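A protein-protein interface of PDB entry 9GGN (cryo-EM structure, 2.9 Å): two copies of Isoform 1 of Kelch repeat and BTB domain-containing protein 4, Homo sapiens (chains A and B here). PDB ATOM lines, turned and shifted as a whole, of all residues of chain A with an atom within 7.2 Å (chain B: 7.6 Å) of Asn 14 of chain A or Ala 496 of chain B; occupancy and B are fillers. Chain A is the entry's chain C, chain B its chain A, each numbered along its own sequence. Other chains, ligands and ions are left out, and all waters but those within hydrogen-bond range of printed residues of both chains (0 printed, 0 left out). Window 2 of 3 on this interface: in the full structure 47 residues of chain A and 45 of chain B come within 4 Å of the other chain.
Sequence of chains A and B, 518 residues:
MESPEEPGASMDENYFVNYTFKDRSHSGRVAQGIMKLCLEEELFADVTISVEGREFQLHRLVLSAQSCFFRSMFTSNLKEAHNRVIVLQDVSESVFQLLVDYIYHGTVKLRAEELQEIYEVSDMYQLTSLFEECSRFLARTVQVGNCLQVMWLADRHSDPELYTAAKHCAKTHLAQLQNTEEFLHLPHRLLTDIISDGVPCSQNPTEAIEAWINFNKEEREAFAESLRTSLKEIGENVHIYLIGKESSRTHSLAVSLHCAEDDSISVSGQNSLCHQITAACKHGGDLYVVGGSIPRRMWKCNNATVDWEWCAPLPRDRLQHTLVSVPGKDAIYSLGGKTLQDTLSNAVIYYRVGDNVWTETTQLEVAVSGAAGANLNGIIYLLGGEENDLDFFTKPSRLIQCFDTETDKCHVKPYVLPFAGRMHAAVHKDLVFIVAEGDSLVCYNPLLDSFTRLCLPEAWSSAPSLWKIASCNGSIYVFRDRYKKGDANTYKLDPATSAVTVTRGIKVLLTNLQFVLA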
ATOM      1  N   GLU A  13     -30.873  -8.680 -16.906  1.00  0.00           N
ATOM      2  CA  GLU A  13     -31.333  -8.664 -18.288  1.00  0.00           C
ATOM      3  C   GLU A  13     -30.333  -7.949 -19.191  1.00  0.00           C
ATOM      4  O   GLU A  13     -29.150  -7.853 -18.866  1.00  0.00           O
ATOM      5  CB  GLU A  13     -32.705  -7.992 -18.390  1.00  0.00           C
ATOM      6  N   ASN A  14     -30.819  -7.452 -20.325  1.00  0.00           N
ATOM      7  CA  ASN A  14     -29.958  -6.759 -21.274  1.00  0.00           C
ATOM      8  C   ASN A  14     -29.458  -5.458 -20.659  1.00  0.00           C
ATOM      9  O   ASN A  14     -30.249  -4.631 -20.197  1.00  0.00           O
ATOM     10  CB  ASN A  14     -30.721  -6.487 -22.572  1.00  0.00           C
ATOM     11  CG  ASN A  14     -29.836  -5.925 -23.679  1.00  0.00           C
ATOM     12  OD1 ASN A  14     -28.868  -5.209 -23.424  1.00  0.00           O
ATOM     13  ND2 ASN A  14     -30.175  -6.253 -24.919  1.00  0.00           N
ATOM     14  N   TYR A  15     -28.137  -5.267 -20.673  1.00  0.00           N
ATOM     15  CA  TYR A  15     -27.540  -4.099 -20.039  1.00  0.00           C
ATOM     16  C   TYR A  15     -27.818  -2.808 -20.792  1.00  0.00           C
ATOM     17  O   TYR A  15     -27.548  -1.729 -20.255  1.00  0.00           O
ATOM     18  CB  TYR A  15     -26.029  -4.288 -19.897  1.00  0.00           C
ATOM     19  CG  TYR A  15     -25.632  -5.389 -18.943  1.00  0.00           C
ATOM     20  CD1 TYR A  15     -26.496  -5.813 -17.943  1.00  0.00           C
ATOM     21  CD2 TYR A  15     -24.392  -6.003 -19.039  1.00  0.00           C
ATOM     22  CE1 TYR A  15     -26.137  -6.818 -17.069  1.00  0.00           C
ATOM     23  CE2 TYR A  15     -24.024  -7.009 -18.170  1.00  0.00           C
ATOM     24  CZ  TYR A  15     -24.900  -7.411 -17.188  1.00  0.00           C
ATOM     25  OH  TYR A  15     -24.537  -8.412 -16.320  1.00  0.00           O
ATOM     26  N   PHE A  16     -28.339  -2.887 -22.013  1.00  0.00           N
ATOM     27  CA  PHE A  16     -28.606  -1.702 -22.814  1.00  0.00           C
ATOM     28  C   PHE A  16     -30.026  -1.180 -22.642  1.00  0.00           C
ATOM     29  O   PHE A  16     -30.361  -0.142 -23.222  1.00  0.00           O
ATOM     30  CB  PHE A  16     -28.342  -1.995 -24.296  1.00  0.00           C
ATOM     31  CG  PHE A  16     -26.891  -2.213 -24.624  1.00  0.00           C
ATOM     32  CD1 PHE A  16     -26.263  -3.403 -24.297  1.00  0.00           C
ATOM     33  CD2 PHE A  16     -26.159  -1.227 -25.261  1.00  0.00           C
ATOM     34  CE1 PHE A  16     -24.929  -3.604 -24.599  1.00  0.00           C
ATOM     35  CE2 PHE A  16     -24.825  -1.423 -25.566  1.00  0.00           C
ATOM     36  CZ  PHE A  16     -24.210  -2.612 -25.235  1.00  0.00           C
ATOM     37  N   VAL A  17     -30.867  -1.867 -21.867  1.00  0.00           N
ATOM     38  CA  VAL A  17     -32.230  -1.403 -21.635  1.00  0.00           C
ATOM     39  C   VAL A  17     -32.509  -1.277 -20.140  1.00  0.00           C
ATOM     40  O   VAL A  17     -33.036  -0.252 -19.690  1.00  0.00           O
ATOM     41  CB  VAL A  17     -33.258  -2.319 -22.331  1.00  0.00           C
ATOM     42  CG1 VAL A  17     -33.102  -2.231 -23.839  1.00  0.00           C
ATOM     43  CG2 VAL A  17     -33.100  -3.766 -21.886  1.00  0.00           C
ATOM     44  N   ASN A  18     -32.154  -2.298 -19.359  1.00  0.00           N
ATOM     45  CA  ASN A  18     -32.376  -2.266 -17.919  1.00  0.00           C
ATOM     46  C   ASN A  18     -31.613  -3.402 -17.250  1.00  0.00           C
ATOM     47  O   ASN A  18     -31.507  -4.496 -17.806  1.00  0.00           O
ATOM     48  CB  ASN A  18     -33.877  -2.348 -17.582  1.00  0.00           C
ATOM     49  CG  ASN A  18     -34.483  -3.710 -17.881  1.00  0.00           C
ATOM     50  OD1 ASN A  18     -33.994  -4.454 -18.731  1.00  0.00           O
ATOM     51  ND2 ASN A  18     -35.559  -4.040 -17.178  1.00  0.00           N
ATOM     52  N   TYR A  19     -31.081  -3.131 -16.060  1.00  0.00           N
ATOM     53  CA  TYR A  19     -30.396  -4.155 -15.281  1.00  0.00           C
ATOM     54  C   TYR A  19     -30.342  -3.715 -13.824  1.00  0.00           C
ATOM     55  O   TYR A  19     -30.600  -2.556 -13.492  1.00  0.00           O
ATOM     56  CB  TYR A  19     -28.990  -4.426 -15.829  1.00  0.00           C
ATOM     57  CG  TYR A  19     -28.044  -3.248 -15.742  1.00  0.00           C
ATOM     58  CD1 TYR A  19     -27.269  -3.033 -14.609  1.00  0.00           C
ATOM     59  CD2 TYR A  19     -27.919  -2.355 -16.797  1.00  0.00           C
ATOM     60  CE1 TYR A  19     -26.403  -1.961 -14.528  1.00  0.00           C
ATOM     61  CE2 TYR A  19     -27.055  -1.281 -16.725  1.00  0.00           C
ATOM     62  CZ  TYR A  19     -26.301  -1.088 -15.589  1.00  0.00           C
ATOM     63  OH  TYR A  19     -25.439  -0.018 -15.515  1.00  0.00           O
ATOM     64  N   LEU B 110     -32.120   0.078 -12.746  1.00  0.00           N
ATOM     65  CA  LEU B 110     -32.251   1.216 -13.642  1.00  0.00           C
ATOM     66  C   LEU B 110     -32.766   0.769 -15.006  1.00  0.00           C
ATOM     67  O   LEU B 110     -32.659  -0.397 -15.391  1.00  0.00           O
ATOM     68  CB  LEU B 110     -30.917   1.946 -13.798  1.00  0.00           C
ATOM     69  CG  LEU B 110     -30.183   2.320 -12.510  1.00  0.00           C
ATOM     70  CD1 LEU B 110     -29.086   1.319 -12.212  1.00  0.00           C
ATOM     71  CD2 LEU B 110     -29.614   3.726 -12.606  1.00  0.00           C
ATOM     72  N   PHE B 137     -23.198   4.155 -18.282  1.00  0.00           N
ATOM     73  CA  PHE B 137     -24.391   3.816 -19.051  1.00  0.00           C
ATOM     74  C   PHE B 137     -24.475   4.659 -20.318  1.00  0.00           C
ATOM     75  O   PHE B 137     -24.761   4.144 -21.405  1.00  0.00           O
ATOM     76  CB  PHE B 137     -25.637   4.010 -18.184  1.00  0.00           C
ATOM     77  CG  PHE B 137     -26.811   3.163 -18.595  1.00  0.00           C
ATOM     78  CD1 PHE B 137     -27.342   3.251 -19.872  1.00  0.00           C
ATOM     79  CD2 PHE B 137     -27.393   2.286 -17.695  1.00  0.00           C
ATOM     80  CE1 PHE B 137     -28.422   2.475 -20.243  1.00  0.00           C
ATOM     81  CE2 PHE B 137     -28.473   1.509 -18.061  1.00  0.00           C
ATOM     82  CZ  PHE B 137     -28.988   1.604 -19.336  1.00  0.00           C
ATOM     83  N   ARG B 140     -21.869   3.658 -22.815  1.00  0.00           N
ATOM     84  CA  ARG B 140     -22.152   2.360 -23.414  1.00  0.00           C
ATOM     85  C   ARG B 140     -23.274   2.450 -24.444  1.00  0.00           C
ATOM     86  O   ARG B 140     -23.092   2.092 -25.612  1.00  0.00           O
ATOM     87  CB  ARG B 140     -22.502   1.355 -22.313  1.00  0.00           C
ATOM     88  CG  ARG B 140     -22.859  -0.034 -22.807  1.00  0.00           C
ATOM     89  CD  ARG B 140     -23.564  -0.816 -21.713  1.00  0.00           C
ATOM     90  NE  ARG B 140     -22.796  -0.815 -20.474  1.00  0.00           N
ATOM     91  CZ  ARG B 140     -23.307  -1.064 -19.275  1.00  0.00           C
ATOM     92  NH1 ARG B 140     -24.595  -1.320 -19.113  1.00  0.00           N
ATOM     93  NH2 ARG B 140     -22.508  -1.047 -18.213  1.00  0.00           N
ATOM     94  N   THR B 141     -24.447   2.927 -24.023  1.00  0.00           N
ATOM     95  CA  THR B 141     -25.612   2.951 -24.899  1.00  0.00           C
ATOM     96  C   THR B 141     -25.563   4.085 -25.918  1.00  0.00           C
ATOM     97  O   THR B 141     -26.226   3.987 -26.958  1.00  0.00           O
ATOM     98  CB  THR B 141     -26.883   3.061 -24.048  1.00  0.00           C
ATOM     99  OG1 THR B 141     -26.875   2.032 -23.049  1.00  0.00           O
ATOM    100  CG2 THR B 141     -28.135   2.895 -24.898  1.00  0.00           C
ATOM    101  N   CYS B 443     -22.893 -12.522 -22.487  1.00  0.00           N
ATOM    102  CA  CYS B 443     -22.298 -11.248 -22.124  1.00  0.00           C
ATOM    103  C   CYS B 443     -21.571 -11.369 -20.787  1.00  0.00           C
ATOM    104  O   CYS B 443     -21.824 -12.275 -19.989  1.00  0.00           O
ATOM    105  CB  CYS B 443     -23.369 -10.163 -22.037  1.00  0.00           C
ATOM    106  SG  CYS B 443     -23.578  -9.186 -23.538  1.00  0.00           S
ATOM    107  N   PHE B 451     -23.890 -11.950 -15.968  1.00  0.00           N
ATOM    108  CA  PHE B 451     -24.062 -12.345 -17.357  1.00  0.00           C
ATOM    109  C   PHE B 451     -25.480 -12.027 -17.810  1.00  0.00           C
ATOM    110  O   PHE B 451     -26.423 -12.046 -17.013  1.00  0.00           O
ATOM    111  CB  PHE B 451     -23.787 -13.842 -17.558  1.00  0.00           C
ATOM    112  CG  PHE B 451     -22.555 -14.338 -16.856  1.00  0.00           C
ATOM    113  CD1 PHE B 451     -21.323 -14.305 -17.486  1.00  0.00           C
ATOM    114  CD2 PHE B 451     -22.630 -14.848 -15.571  1.00  0.00           C
ATOM    115  CE1 PHE B 451     -20.190 -14.766 -16.846  1.00  0.00           C
ATOM    116  CE2 PHE B 451     -21.500 -15.307 -14.926  1.00  0.00           C
ATOM    117  CZ  PHE B 451     -20.279 -15.266 -15.564  1.00  0.00           C
ATOM    118  N   THR B 452     -25.623 -11.736 -19.102  1.00  0.00           N
ATOM    119  CA  THR B 452     -26.932 -11.506 -19.698  1.00  0.00           C
ATOM    120  C   THR B 452     -27.510 -12.743 -20.372  1.00  0.00           C
ATOM    121  O   THR B 452     -28.727 -12.947 -20.323  1.00  0.00           O
ATOM    122  CB  THR B 452     -26.847 -10.362 -20.719  1.00  0.00           C
ATOM    123  OG1 THR B 452     -26.484  -9.150 -20.048  1.00  0.00           O
ATOM    124  CG2 THR B 452     -28.179 -10.154 -21.428  1.00  0.00           C
ATOM    125  N   ARG B 453     -26.662 -13.586 -20.964  1.00  0.00           N
ATOM    126  CA  ARG B 453     -27.076 -14.861 -21.553  1.00  0.00           C
ATOM    127  C   ARG B 453     -28.159 -14.653 -22.615  1.00  0.00           C
ATOM    128  O   ARG B 453     -29.294 -15.116 -22.488  1.00  0.00           O
ATOM    129  CB  ARG B 453     -27.549 -15.836 -20.469  1.00  0.00           C
ATOM    130  CG  ARG B 453     -27.489 -17.300 -20.873  1.00  0.00           C
ATOM    131  CD  ARG B 453     -26.336 -18.010 -20.188  1.00  0.00           C
ATOM    132  NE  ARG B 453     -26.710 -18.490 -18.863  1.00  0.00           N
ATOM    133  CZ  ARG B 453     -26.405 -17.876 -17.728  1.00  0.00           C
ATOM    134  NH1 ARG B 453     -25.710 -16.750 -17.716  1.00  0.00           N
ATOM    135  NH2 ARG B 453     -26.804 -18.406 -16.575  1.00  0.00           N
ATOM    136  N   LEU B 454     -27.784 -13.941 -23.674  1.00  0.00           N
ATOM    137  CA  LEU B 454     -28.699 -13.734 -24.784  1.00  0.00           C
ATOM    138  C   LEU B 454     -28.885 -15.031 -25.570  1.00  0.00           C
ATOM    139  O   LEU B 454     -28.198 -16.035 -25.349  1.00  0.00           O
ATOM    140  CB  LEU B 454     -28.190 -12.624 -25.700  1.00  0.00           C
ATOM    141  N   LEU B 493     -24.472  -7.410 -35.461  1.00  0.00           N
ATOM    142  CA  LEU B 493     -25.378  -7.633 -34.346  1.00  0.00           C
ATOM    143  C   LEU B 493     -25.685  -6.313 -33.652  1.00  0.00           C
ATOM    144  O   LEU B 493     -24.852  -5.401 -33.619  1.00  0.00           O
ATOM    145  CB  LEU B 493     -24.783  -8.639 -33.347  1.00  0.00           C
ATOM    146  CG  LEU B 493     -25.633  -9.095 -32.157  1.00  0.00           C
ATOM    147  CD1 LEU B 493     -25.361 -10.556 -31.856  1.00  0.00           C
ATOM    148  CD2 LEU B 493     -25.356  -8.249 -30.923  1.00  0.00           C
ATOM    149  N   ASP B 494     -26.888  -6.220 -33.097  1.00  0.00           N
ATOM    150  CA  ASP B 494     -27.306  -5.065 -32.303  1.00  0.00           C
ATOM    151  C   ASP B 494     -27.728  -5.534 -30.919  1.00  0.00           C
ATOM    152  O   ASP B 494     -28.819  -6.119 -30.773  1.00  0.00           O
ATOM    153  CB  ASP B 494     -28.453  -4.321 -32.988  1.00  0.00           C
ATOM    154  N   PRO B 495     -26.920  -5.307 -29.879  1.00  0.00           N
ATOM    155  CA  PRO B 495     -27.241  -5.861 -28.557  1.00  0.00           C
ATOM    156  C   PRO B 495     -28.342  -5.120 -27.816  1.00  0.00           C
ATOM    157  O   PRO B 495     -28.774  -5.601 -26.759  1.00  0.00           O
ATOM    158  CB  PRO B 495     -25.909  -5.747 -27.807  1.00  0.00           C
ATOM    159  CG  PRO B 495     -25.262  -4.546 -28.409  1.00  0.00           C
ATOM    160  CD  PRO B 495     -25.666  -4.533 -29.865  1.00  0.00           C
ATOM    161  N   ALA B 496     -28.799  -3.972 -28.319  1.00  0.00           N
ATOM    162  CA  ALA B 496     -29.814  -3.202 -27.606  1.00  0.00           C
ATOM    163  C   ALA B 496     -31.117  -3.984 -27.498  1.00  0.00           C
ATOM    164  O   ALA B 496     -31.729  -4.052 -26.426  1.00  0.00           O
ATOM    165  CB  ALA B 496     -30.043  -1.863 -28.306  1.00  0.00           C
ATOM    166  N   THR B 497     -31.558  -4.584 -28.603  1.00  0.00           N
ATOM    167  CA  THR B 497     -32.801  -5.345 -28.640  1.00  0.00           C
ATOM    168  C   THR B 497     -32.565  -6.818 -28.947  1.00  0.00           C
ATOM    169  O   THR B 497     -33.523  -7.536 -29.256  1.00  0.00           O
ATOM    170  CB  THR B 497     -33.766  -4.748 -29.669  1.00  0.00           C
ATOM    171  N   SER B 498     -31.316  -7.282 -28.870  1.00  0.00           N
ATOM    172  CA  SER B 498     -30.943  -8.654 -29.219  1.00  0.00           C
ATOM    173  C   SER B 498     -31.371  -9.010 -30.640  1.00  0.00           C
ATOM    174  O   SER B 498     -31.687 -10.165 -30.935  1.00  0.00           O
ATOM    175  CB  SER B 498     -31.516  -9.662 -28.219  1.00  0.00           C
ATOM    176  OG  SER B 498     -31.050 -10.972 -28.491  1.00  0.00           O
ATOM    177  N   ALA B 499     -31.382  -8.021 -31.530  1.00  0.00           N
ATOM    178  CA  ALA B 499     -31.786  -8.212 -32.915  1.00  0.00           C
ATOM    179  C   ALA B 499     -30.552  -8.251 -33.806  1.00  0.00           C
ATOM    180  O   ALA B 499     -29.670  -7.395 -33.689  1.00  0.00           O
ATOM    181  CB  ALA B 499     -32.731  -7.098 -33.367  1.00  0.00           C
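The backbone NH (N) of Leu 110 of chain B is in hydrogen-bond range of the backbone carbonyl oxygen (O) of Tyr 19 of chain A (3.1 Å). The backbone carbonyl oxygen of Pro 495 of chain B sits at hydrogen-bond distance from the side-chain amide nitrogen of Asn 14 of chain A (2.4 Å). NH1 of Arg 140 of chain B sits at hydrogen-bond distance from O of Tyr 15 of chain A (3.2 Å). ND2 of Asn 14 of chain A lies within hydrogen-bond range of O of Ala 496 of chain B, 3.1 Å away. The side-chain hydroxyl of Thr 452 of chain B sits at hydrogen-bond distance from the backbone carbonyl oxygen of Glu 13 of chain A.
The backbone NH (N) of Phe 16 of chain A is in hydrogen-bond range of the side-chain amide oxygen (OD1) of Asn 14 of chain A. The backbone carbonyl oxygen of Phe 137 of chain B lies close to the side-chain hydroxyl of Thr 141 of chain B, 3.4 Å away.
Among the printed residues, merely in contact across the chains: Asn 14 of chain A with Thr 452 of chain B (3.8 Å), Tyr 15 of chain A with Phe 137 of chain B (3.7 Å), Tyr 15 of chain A with Phe 451 of chain B (3.6 Å), Tyr 15 of chain A with Thr 452 of chain B (3.7 Å), Phe 16 of chain A with Arg 140 of chain B (3.7 Å), Phe 16 of chain A with Pro 495 of chain B (3.9 Å), Phe 16 of chain A with Ala 496 of chain B (3.8 Å), Val 17 of chain A with Ala 496 of chain B (3.4 Å), Asn 18 of chain A with Leu 110 of chain B (3.2 Å), Tyr 19 of chain A with Phe 137 of chain B (3.4 Å) and Tyr 19 of chain A with Arg 140 of chain B (3.4 Å).
Of the printed residues of chain B, Glu 13 of chain A touches Thr 452. Printed residues of chain B within 4 Å of Asn 14 of chain A: Thr 452, Pro 495 and Ala 496. Of the printed residues of chain B, Phe 16 of chain A touches Arg 140, Pro 495 and Ala 496. Printed residues of chain A within 4 Å of Phe 137 of chain B: Tyr 15 (3.7 Å) and Tyr 19 (3.4 Å). Printed residues of chain A within 4 Å of Arg 140 of chain B: Tyr 15 (3.2 Å), Phe 16 (3.7 Å) and Tyr 19 (3.4 Å). Of the printed residues of chain A, Pro 495 of chain B touches Asn 14 (2.4 Å) and Phe 16 (3.9 Å). The nearest residue of chain A that does not touch Ala 496 of chain B is Tyr 15 of chain A (6.9 Å). The nearest printed residue of chain A that does not touch Phe 451 of chain B is Glu 13 of chain A (5.3 Å).
Of the 16 printed residues of chain B, 7 touch a printed residue of chain A. Hydrophobic or aromatic side chains of chain B within 4 Å of the printed part of chain A: Phe 137 and Pro 495. Among the printed residues, 16 pairs touch across the chains. Among the printed residues, no Asp or Glu carboxylate lies within 4 Å of a Lys or Arg side-chain nitrogen of the other chain.
No position is printed for both chains.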
